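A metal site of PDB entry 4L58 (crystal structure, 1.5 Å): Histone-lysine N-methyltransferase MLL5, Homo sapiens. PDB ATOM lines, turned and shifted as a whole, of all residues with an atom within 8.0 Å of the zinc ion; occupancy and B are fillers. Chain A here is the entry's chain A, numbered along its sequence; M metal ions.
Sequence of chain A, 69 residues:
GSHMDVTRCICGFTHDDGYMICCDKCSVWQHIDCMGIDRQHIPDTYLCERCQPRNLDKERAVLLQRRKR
ND1 of His 31 is bound to the zinc ion (2.1 Å). SG of Cys 34 is bound to the zinc ion (2.3 Å). The zinc ion is bound by SG of Cys 9 (2.3 Å). The zinc ion is bound by SG of Cys 11 (2.3 Å). The zinc ion has four donor atoms within binding distance.
CG of Gln 65 touches the zinc ion (3.8 Å). Of the 26 residues printed, 5 come within 4 Å of the zinc ion. The nearest printed residue that does not touch the zinc ion is Ile 10 (4.7 Å).
The side-chain sulfur of Cys 34 lies close to the side-chain amide nitrogen of Gln 65, at 3.4 Å. NE2 of Gln 65 lies within hydrogen-bond range of OD1 of Asp 17 (2.9 Å). NE2 of His 15 sits at hydrogen-bond distance from OE1 of Gln 65, at 2.8 Å. A ring nitrogen (NE2) of His 31 sits at hydrogen-bond distance from the backbone carbonyl oxygen of His 15 (2.8 Å). SG of Cys 11 lies close to N of Phe 13.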
ATOM      1  N   THR A   7       0.680  23.651  24.699  1.00  0.00           N
ATOM      2  CA  THR A   7       0.991  23.646  23.272  1.00  0.00           C
ATOM      3  C   THR A   7       2.478  23.357  23.081  1.00  0.00           C
ATOM      4  O   THR A   7       3.330  24.036  23.668  1.00  0.00           O
ATOM      5  CB  THR A   7       0.640  24.990  22.612  1.00  0.00           C
ATOM      6  OG1 THR A   7      -0.789  25.145  22.592  1.00  0.00           O
ATOM      7  CG2 THR A   7       1.170  25.073  21.190  1.00  0.00           C
ATOM      8  N   ARG A   8       2.777  22.348  22.283  1.00  0.00           N
ATOM      9  CA  ARG A   8       4.159  22.062  21.893  1.00  0.00           C
ATOM     10  C   ARG A   8       4.157  21.504  20.478  1.00  0.00           C
ATOM     11  O   ARG A   8       3.966  20.312  20.267  1.00  0.00           O
ATOM     12  CB  ARG A   8       4.839  21.062  22.822  1.00  0.00           C
ATOM     13  CG  ARG A   8       6.331  20.922  22.538  1.00  0.00           C
ATOM     14  CD  ARG A   8       6.940  19.652  23.121  1.00  0.00           C
ATOM     15  NE  ARG A   8       6.359  18.452  22.530  1.00  0.00           N
ATOM     16  CZ  ARG A   8       6.581  18.051  21.285  1.00  0.00           C
ATOM     17  NH1 ARG A   8       7.383  18.739  20.475  1.00  0.00           N
ATOM     18  NH2 ARG A   8       6.001  16.942  20.839  1.00  0.00           N
ATOM     19  N   CYS A   9       4.376  22.389  19.512  1.00  0.00           N
ATOM     20  CA  CYS A   9       4.376  22.028  18.107  1.00  0.00           C
ATOM     21  C   CYS A   9       5.794  22.117  17.557  1.00  0.00           C
ATOM     22  O   CYS A   9       6.665  22.739  18.165  1.00  0.00           O
ATOM     23  CB  CYS A   9       3.435  22.960  17.343  1.00  0.00           C
ATOM     24  SG  CYS A   9       3.115  22.453  15.646  1.00  0.00           S
ATOM     25  N   ILE A  10       6.034  21.484  16.411  1.00  0.00           N
ATOM     26  CA  ILE A  10       7.378  21.467  15.851  1.00  0.00           C
ATOM     27  C   ILE A  10       7.820  22.849  15.390  1.00  0.00           C
ATOM     28  O   ILE A  10       9.013  23.089  15.233  1.00  0.00           O
ATOM     29  CB  ILE A  10       7.538  20.448  14.702  1.00  0.00           C
ATOM     30  CG1 ILE A  10       6.636  20.797  13.515  1.00  0.00           C
ATOM     31  CG2 ILE A  10       7.235  19.038  15.190  1.00  0.00           C
ATOM     32  CD1 ILE A  10       6.914  19.942  12.291  1.00  0.00           C
ATOM     33  N   CYS A  11       6.873  23.767  15.181  1.00  0.00           N
ATOM     34  CA  CYS A  11       7.205  25.138  14.776  1.00  0.00           C
ATOM     35  C   CYS A  11       7.728  25.974  15.931  1.00  0.00           C
ATOM     36  O   CYS A  11       8.376  27.010  15.727  1.00  0.00           O
ATOM     37  CB  CYS A  11       5.971  25.832  14.197  1.00  0.00           C
ATOM     38  SG  CYS A  11       4.619  26.012  15.369  1.00  0.00           S
ATOM     39  N   GLY A  12       7.428  25.554  17.159  1.00  0.00           N
ATOM     40  CA  GLY A  12       7.832  26.284  18.343  1.00  0.00           C
ATOM     41  C   GLY A  12       6.908  27.427  18.740  1.00  0.00           C
ATOM     42  O   GLY A  12       7.065  28.015  19.811  1.00  0.00           O
ATOM     43  N   PHE A  13       5.938  27.752  17.886  1.00  0.00           N
ATOM     44  CA  PHE A  13       5.014  28.837  18.208  1.00  0.00           C
ATOM     45  C   PHE A  13       3.934  28.365  19.169  1.00  0.00           C
ATOM     46  O   PHE A  13       3.485  27.216  19.100  1.00  0.00           O
ATOM     47  CB  PHE A  13       4.362  29.418  16.964  1.00  0.00           C
ATOM     48  CG  PHE A  13       5.291  30.245  16.123  1.00  0.00           C
ATOM     49  CD1 PHE A  13       5.653  31.525  16.520  1.00  0.00           C
ATOM     50  CD2 PHE A  13       5.797  29.752  14.931  1.00  0.00           C
ATOM     51  CE1 PHE A  13       6.513  32.290  15.748  1.00  0.00           C
ATOM     52  CE2 PHE A  13       6.647  30.513  14.156  1.00  0.00           C
ATOM     53  CZ  PHE A  13       7.001  31.783  14.559  1.00  0.00           C
ATOM     54  N   THR A  14       3.508  29.256  20.046  1.00  0.00           N
ATOM     55  CA  THR A  14       2.592  28.903  21.118  1.00  0.00           C
ATOM     56  C   THR A  14       1.168  29.419  20.870  1.00  0.00           C
ATOM     57  O   THR A  14       0.261  29.106  21.632  1.00  0.00           O
ATOM     58  CB  THR A  14       3.095  29.427  22.475  1.00  0.00           C
ATOM     59  OG1 THR A  14       3.243  30.854  22.423  1.00  0.00           O
ATOM     60  CG2 THR A  14       4.433  28.801  22.808  1.00  0.00           C
ATOM     61  N   HIS A  15       0.981  30.205  19.824  1.00  0.00           N
ATOM     62  CA  HIS A  15      -0.355  30.700  19.487  1.00  0.00           C
ATOM     63  C   HIS A  15      -1.231  29.572  18.963  1.00  0.00           C
ATOM     64  O   HIS A  15      -0.738  28.524  18.556  1.00  0.00           O
ATOM     65  CB  HIS A  15      -0.301  31.825  18.456  1.00  0.00           C
ATOM     66  CG  HIS A  15       0.309  31.418  17.151  1.00  0.00           C
ATOM     67  ND1 HIS A  15       1.640  31.633  16.855  1.00  0.00           N
ATOM     68  CD2 HIS A  15      -0.220  30.815  16.066  1.00  0.00           C
ATOM     69  CE1 HIS A  15       1.903  31.169  15.640  1.00  0.00           C
ATOM     70  NE2 HIS A  15       0.785  30.664  15.138  1.00  0.00           N
ATOM     71  N   ASP A  17      -3.636  28.549  15.987  1.00  0.00           N
ATOM     72  CA  ASP A  17      -3.813  28.979  14.595  1.00  0.00           C
ATOM     73  C   ASP A  17      -5.167  28.616  13.990  1.00  0.00           C
ATOM     74  O   ASP A  17      -5.374  28.790  12.789  1.00  0.00           O
ATOM     75  CB  ASP A  17      -2.685  28.412  13.712  1.00  0.00           C
ATOM     76  CG  ASP A  17      -2.892  26.948  13.369  1.00  0.00           C
ATOM     77  OD1 ASP A  17      -2.303  26.475  12.381  1.00  0.00           O
ATOM     78  OD2 ASP A  17      -3.641  26.271  14.090  1.00  0.00           O
ATOM     79  N   TYR A  19      -6.678  25.521  13.915  1.00  0.00           N
ATOM     80  CA  TYR A  19      -6.892  24.091  13.714  1.00  0.00           C
ATOM     81  C   TYR A  19      -5.749  23.279  14.325  1.00  0.00           C
ATOM     82  O   TYR A  19      -4.682  23.119  13.726  1.00  0.00           O
ATOM     83  CB  TYR A  19      -7.082  23.744  12.239  1.00  0.00           C
ATOM     84  CG  TYR A  19      -8.016  22.570  12.010  1.00  0.00           C
ATOM     85  CD1 TYR A  19      -7.970  21.443  12.833  1.00  0.00           C
ATOM     86  CD2 TYR A  19      -8.951  22.585  10.985  1.00  0.00           C
ATOM     87  CE1 TYR A  19      -8.820  20.375  12.624  1.00  0.00           C
ATOM     88  CE2 TYR A  19      -9.806  21.529  10.772  1.00  0.00           C
ATOM     89  CZ  TYR A  19      -9.747  20.423  11.597  1.00  0.00           C
ATOM     90  OH  TYR A  19     -10.589  19.358  11.390  1.00  0.00           O
ATOM     91  N   MET A  20      -5.994  22.772  15.531  1.00  0.00           N
ATOM     92  CA  MET A  20      -4.967  22.081  16.296  1.00  0.00           C
ATOM     93  C   MET A  20      -5.437  20.683  16.676  1.00  0.00           C
ATOM     94  O   MET A  20      -6.623  20.375  16.619  1.00  0.00           O
ATOM     95  CB  MET A  20      -4.618  22.900  17.540  1.00  0.00           C
ATOM     96  CG  MET A  20      -4.057  24.277  17.193  1.00  0.00           C
ATOM     97  SD  MET A  20      -3.358  25.194  18.567  1.00  0.00           S
ATOM     98  CE  MET A  20      -1.877  24.226  18.873  1.00  0.00           C
ATOM     99  N   TRP A  29      -0.734  20.047  22.411  1.00  0.00           N
ATOM    100  CA  TRP A  29      -1.463  20.460  21.225  1.00  0.00           C
ATOM    101  C   TRP A  29      -0.486  20.904  20.152  1.00  0.00           C
ATOM    102  O   TRP A  29       0.533  21.530  20.448  1.00  0.00           O
ATOM    103  CB  TRP A  29      -2.406  21.610  21.555  1.00  0.00           C
ATOM    104  CG  TRP A  29      -3.565  21.191  22.384  1.00  0.00           C
ATOM    105  CD1 TRP A  29      -3.617  21.133  23.740  1.00  0.00           C
ATOM    106  CD2 TRP A  29      -4.835  20.767  21.904  1.00  0.00           C
ATOM    107  NE1 TRP A  29      -4.858  20.699  24.141  1.00  0.00           N
ATOM    108  CE2 TRP A  29      -5.630  20.465  23.031  1.00  0.00           C
ATOM    109  CE3 TRP A  29      -5.391  20.601  20.630  1.00  0.00           C
ATOM    110  CZ2 TRP A  29      -6.935  20.018  22.933  1.00  0.00           C
ATOM    111  CZ3 TRP A  29      -6.688  20.163  20.526  1.00  0.00           C
ATOM    112  CH2 TRP A  29      -7.455  19.867  21.668  1.00  0.00           C
ATOM    113  N   GLN A  30      -0.816  20.582  18.913  1.00  0.00           N
ATOM    114  CA  GLN A  30       0.031  20.918  17.784  1.00  0.00           C
ATOM    115  C   GLN A  30      -0.841  21.442  16.664  1.00  0.00           C
ATOM    116  O   GLN A  30      -2.037  21.155  16.609  1.00  0.00           O
ATOM    117  CB  GLN A  30       0.809  19.683  17.330  1.00  0.00           C
ATOM    118  CG  GLN A  30       1.462  18.924  18.479  1.00  0.00           C
ATOM    119  CD  GLN A  30       2.485  17.936  18.003  1.00  0.00           C
ATOM    120  OE1 GLN A  30       2.156  16.944  17.352  1.00  0.00           O
ATOM    121  NE2 GLN A  30       3.760  18.211  18.288  1.00  0.00           N
ATOM    122  N   HIS A  31      -0.266  22.242  15.765  1.00  0.00           N
ATOM    123  CA  HIS A  31      -1.010  22.762  14.627  1.00  0.00           C
ATOM    124  C   HIS A  31      -1.084  21.700  13.551  1.00  0.00           C
ATOM    125  O   HIS A  31      -0.066  21.130  13.172  1.00  0.00           O
ATOM    126  CB  HIS A  31      -0.320  24.005  14.055  1.00  0.00           C
ATOM    127  CG  HIS A  31       0.000  25.051  15.079  1.00  0.00           C
ATOM    128  ND1 HIS A  31       1.283  25.409  15.407  1.00  0.00           N
ATOM    129  CD2 HIS A  31      -0.815  25.824  15.839  1.00  0.00           C
ATOM    130  CE1 HIS A  31       1.260  26.345  16.341  1.00  0.00           C
ATOM    131  NE2 HIS A  31      -0.007  26.619  16.613  1.00  0.00           N
ATOM    132  N   ILE A  32      -2.277  21.403  13.033  1.00  0.00           N
ATOM    133  CA  ILE A  32      -2.364  20.331  12.059  1.00  0.00           C
ATOM    134  C   ILE A  32      -1.544  20.655  10.803  1.00  0.00           C
ATOM    135  O   ILE A  32      -0.967  19.761  10.207  1.00  0.00           O
ATOM    136  CB  ILE A  32      -3.803  19.925  11.680  1.00  0.00           C
ATOM    137  CG1 ILE A  32      -4.571  21.051  11.005  1.00  0.00           C
ATOM    138  CG2 ILE A  32      -4.543  19.407  12.914  1.00  0.00           C
ATOM    139  CD1 ILE A  32      -5.742  20.529  10.181  1.00  0.00           C
ATOM    140  N   ASP A  33      -1.475  21.927  10.409  1.00  0.00           N
ATOM    141  CA  ASP A  33      -0.713  22.269   9.213  1.00  0.00           C
ATOM    142  C   ASP A  33       0.757  21.904   9.380  1.00  0.00           C
ATOM    143  O   ASP A  33       1.367  21.318   8.497  1.00  0.00           O
ATOM    144  CB  ASP A  33      -0.834  23.764   8.877  1.00  0.00           C
ATOM    145  CG  ASP A  33      -2.189  24.139   8.341  1.00  0.00           C
ATOM    146  OD1 ASP A  33      -3.029  23.245   8.103  1.00  0.00           O
ATOM    147  OD2 ASP A  33      -2.425  25.355   8.133  1.00  0.00           O
ATOM    148  N   CYS A  34       1.309  22.255  10.537  1.00  0.00           N
ATOM    149  CA  CYS A  34       2.699  21.965  10.841  1.00  0.00           C
ATOM    150  C   CYS A  34       2.998  20.474  10.792  1.00  0.00           C
ATOM    151  O   CYS A  34       4.053  20.063  10.314  1.00  0.00           O
ATOM    152  CB  CYS A  34       3.059  22.491  12.226  1.00  0.00           C
ATOM    153  SG  CYS A  34       2.972  24.273  12.355  1.00  0.00           S
ATOM    154  N   MET A  35       2.064  19.683  11.297  1.00  0.00           N
ATOM    155  CA  MET A  35       2.275  18.249  11.444  1.00  0.00           C
ATOM    156  C   MET A  35       1.898  17.484  10.176  1.00  0.00           C
ATOM    157  O   MET A  35       2.001  16.263  10.132  1.00  0.00           O
ATOM    158  CB  MET A  35       1.499  17.726  12.652  1.00  0.00           C
ATOM    159  CG  MET A  35       1.814  18.461  13.949  1.00  0.00           C
ATOM    160  SD  MET A  35       3.580  18.564  14.312  1.00  0.00           S
ATOM    161  CE  MET A  35       3.976  16.834  14.583  1.00  0.00           C
ATOM    162  N   LYS A  58      10.505  20.981   9.764  1.00  0.00           N
ATOM    163  CA  LYS A  58      10.325  21.981  10.804  1.00  0.00           C
ATOM    164  C   LYS A  58      10.332  23.388  10.214  1.00  0.00           C
ATOM    165  O   LYS A  58       9.574  24.253  10.650  1.00  0.00           O
ATOM    166  CB  LYS A  58      11.425  21.801  11.860  1.00  0.00           C
ATOM    167  CG  LYS A  58      11.499  22.893  12.932  1.00  0.00           C
ATOM    168  CD  LYS A  58      12.446  22.500  14.065  1.00  0.00           C
ATOM    169  CE  LYS A  58      12.046  21.218  14.796  1.00  0.00           C
ATOM    170  NZ  LYS A  58      11.092  21.391  15.918  1.00  0.00           N
ATOM    171  N   ARG A  60       9.334  24.344   7.246  1.00  0.00           N
ATOM    172  CA  ARG A  60       8.029  24.557   6.614  1.00  0.00           C
ATOM    173  C   ARG A  60       7.013  24.979   7.651  1.00  0.00           C
ATOM    174  O   ARG A  60       6.218  25.901   7.453  1.00  0.00           O
ATOM    175  CB  ARG A  60       7.551  23.279   5.932  1.00  0.00           C
ATOM    176  CG  ARG A  60       6.090  23.338   5.466  1.00  0.00           C
ATOM    177  CD  ARG A  60       5.673  22.002   4.864  1.00  0.00           C
ATOM    178  NE  ARG A  60       4.234  21.947   4.585  1.00  0.00           N
ATOM    179  CZ  ARG A  60       3.302  21.636   5.481  1.00  0.00           C
ATOM    180  NH1 ARG A  60       3.637  21.368   6.736  1.00  0.00           N
ATOM    181  NH2 ARG A  60       2.023  21.616   5.137  1.00  0.00           N
ATOM    182  N   ALA A  61       7.020  24.297   8.782  1.00  0.00           N
ATOM    183  CA  ALA A  61       6.073  24.591   9.852  1.00  0.00           C
ATOM    184  C   ALA A  61       6.255  26.033  10.325  1.00  0.00           C
ATOM    185  O   ALA A  61       5.288  26.784  10.463  1.00  0.00           O
ATOM    186  CB  ALA A  61       6.260  23.620  10.992  1.00  0.00           C
ATOM    187  N   VAL A  62       7.509  26.417  10.551  1.00  0.00           N
ATOM    188  CA  VAL A  62       7.804  27.764  11.006  1.00  0.00           C
ATOM    189  C   VAL A  62       7.341  28.824  10.004  1.00  0.00           C
ATOM    190  O   VAL A  62       6.714  29.808  10.385  1.00  0.00           O
ATOM    191  CB  VAL A  62       9.308  27.940  11.304  1.00  0.00           C
ATOM    192  CG1 VAL A  62       9.635  29.389  11.599  1.00  0.00           C
ATOM    193  CG2 VAL A  62       9.704  27.056  12.485  1.00  0.00           C
ATOM    194  N   LEU A  64       5.027  28.629   7.708  1.00  0.00           N
ATOM    195  CA  LEU A  64       3.572  28.657   7.652  1.00  0.00           C
ATOM    196  C   LEU A  64       2.986  29.421   8.834  1.00  0.00           C
ATOM    197  O   LEU A  64       2.020  30.167   8.680  1.00  0.00           O
ATOM    198  CB  LEU A  64       2.979  27.253   7.611  1.00  0.00           C
ATOM    199  CG  LEU A  64       3.206  26.473   6.330  1.00  0.00           C
ATOM    200  CD1 LEU A  64       2.647  25.065   6.465  1.00  0.00           C
ATOM    201  CD2 LEU A  64       2.575  27.201   5.148  1.00  0.00           C
ATOM    202  N   GLN A  65       3.564  29.230  10.014  1.00  0.00           N
ATOM    203  CA  GLN A  65       2.985  29.833  11.220  1.00  0.00           C
ATOM    204  C   GLN A  65       3.314  31.320  11.360  1.00  0.00           C
ATOM    205  O   GLN A  65       2.551  32.060  11.978  1.00  0.00           O
ATOM    206  CB  GLN A  65       3.421  29.055  12.459  1.00  0.00           C
ATOM    207  CG  GLN A  65       2.763  27.694  12.555  1.00  0.00           C
ATOM    208  CD  GLN A  65       1.246  27.779  12.599  1.00  0.00           C
ATOM    209  OE1 GLN A  65       0.673  28.783  13.039  1.00  0.00           O
ATOM    210  NE2 GLN A  65       0.589  26.725  12.143  1.00  0.00           N
ATOM    211  N   LYS A  68       0.636  33.547  10.296  1.00  0.00           N
ATOM    212  CA  LYS A  68      -0.622  33.373  11.015  1.00  0.00           C
ATOM    213  C   LYS A  68      -0.664  34.145  12.334  1.00  0.00           C
ATOM    214  O   LYS A  68      -1.660  34.086  13.062  1.00  0.00           O
ATOM    215  CB  LYS A  68      -0.877  31.892  11.310  1.00  0.00           C
ATOM    216  CG  LYS A  68      -1.038  31.021  10.075  1.00  0.00           C
ATOM    217  CD  LYS A  68      -1.445  29.620  10.475  1.00  0.00           C
ATOM    218  CE  LYS A  68      -1.829  28.766   9.292  1.00  0.00           C
ATOM    219  NZ  LYS A  68      -2.489  27.508   9.733  1.00  0.00           N
HETATM  220 ZN    ZN M   1       2.999  24.516  14.617  1.00  0.00          ZN
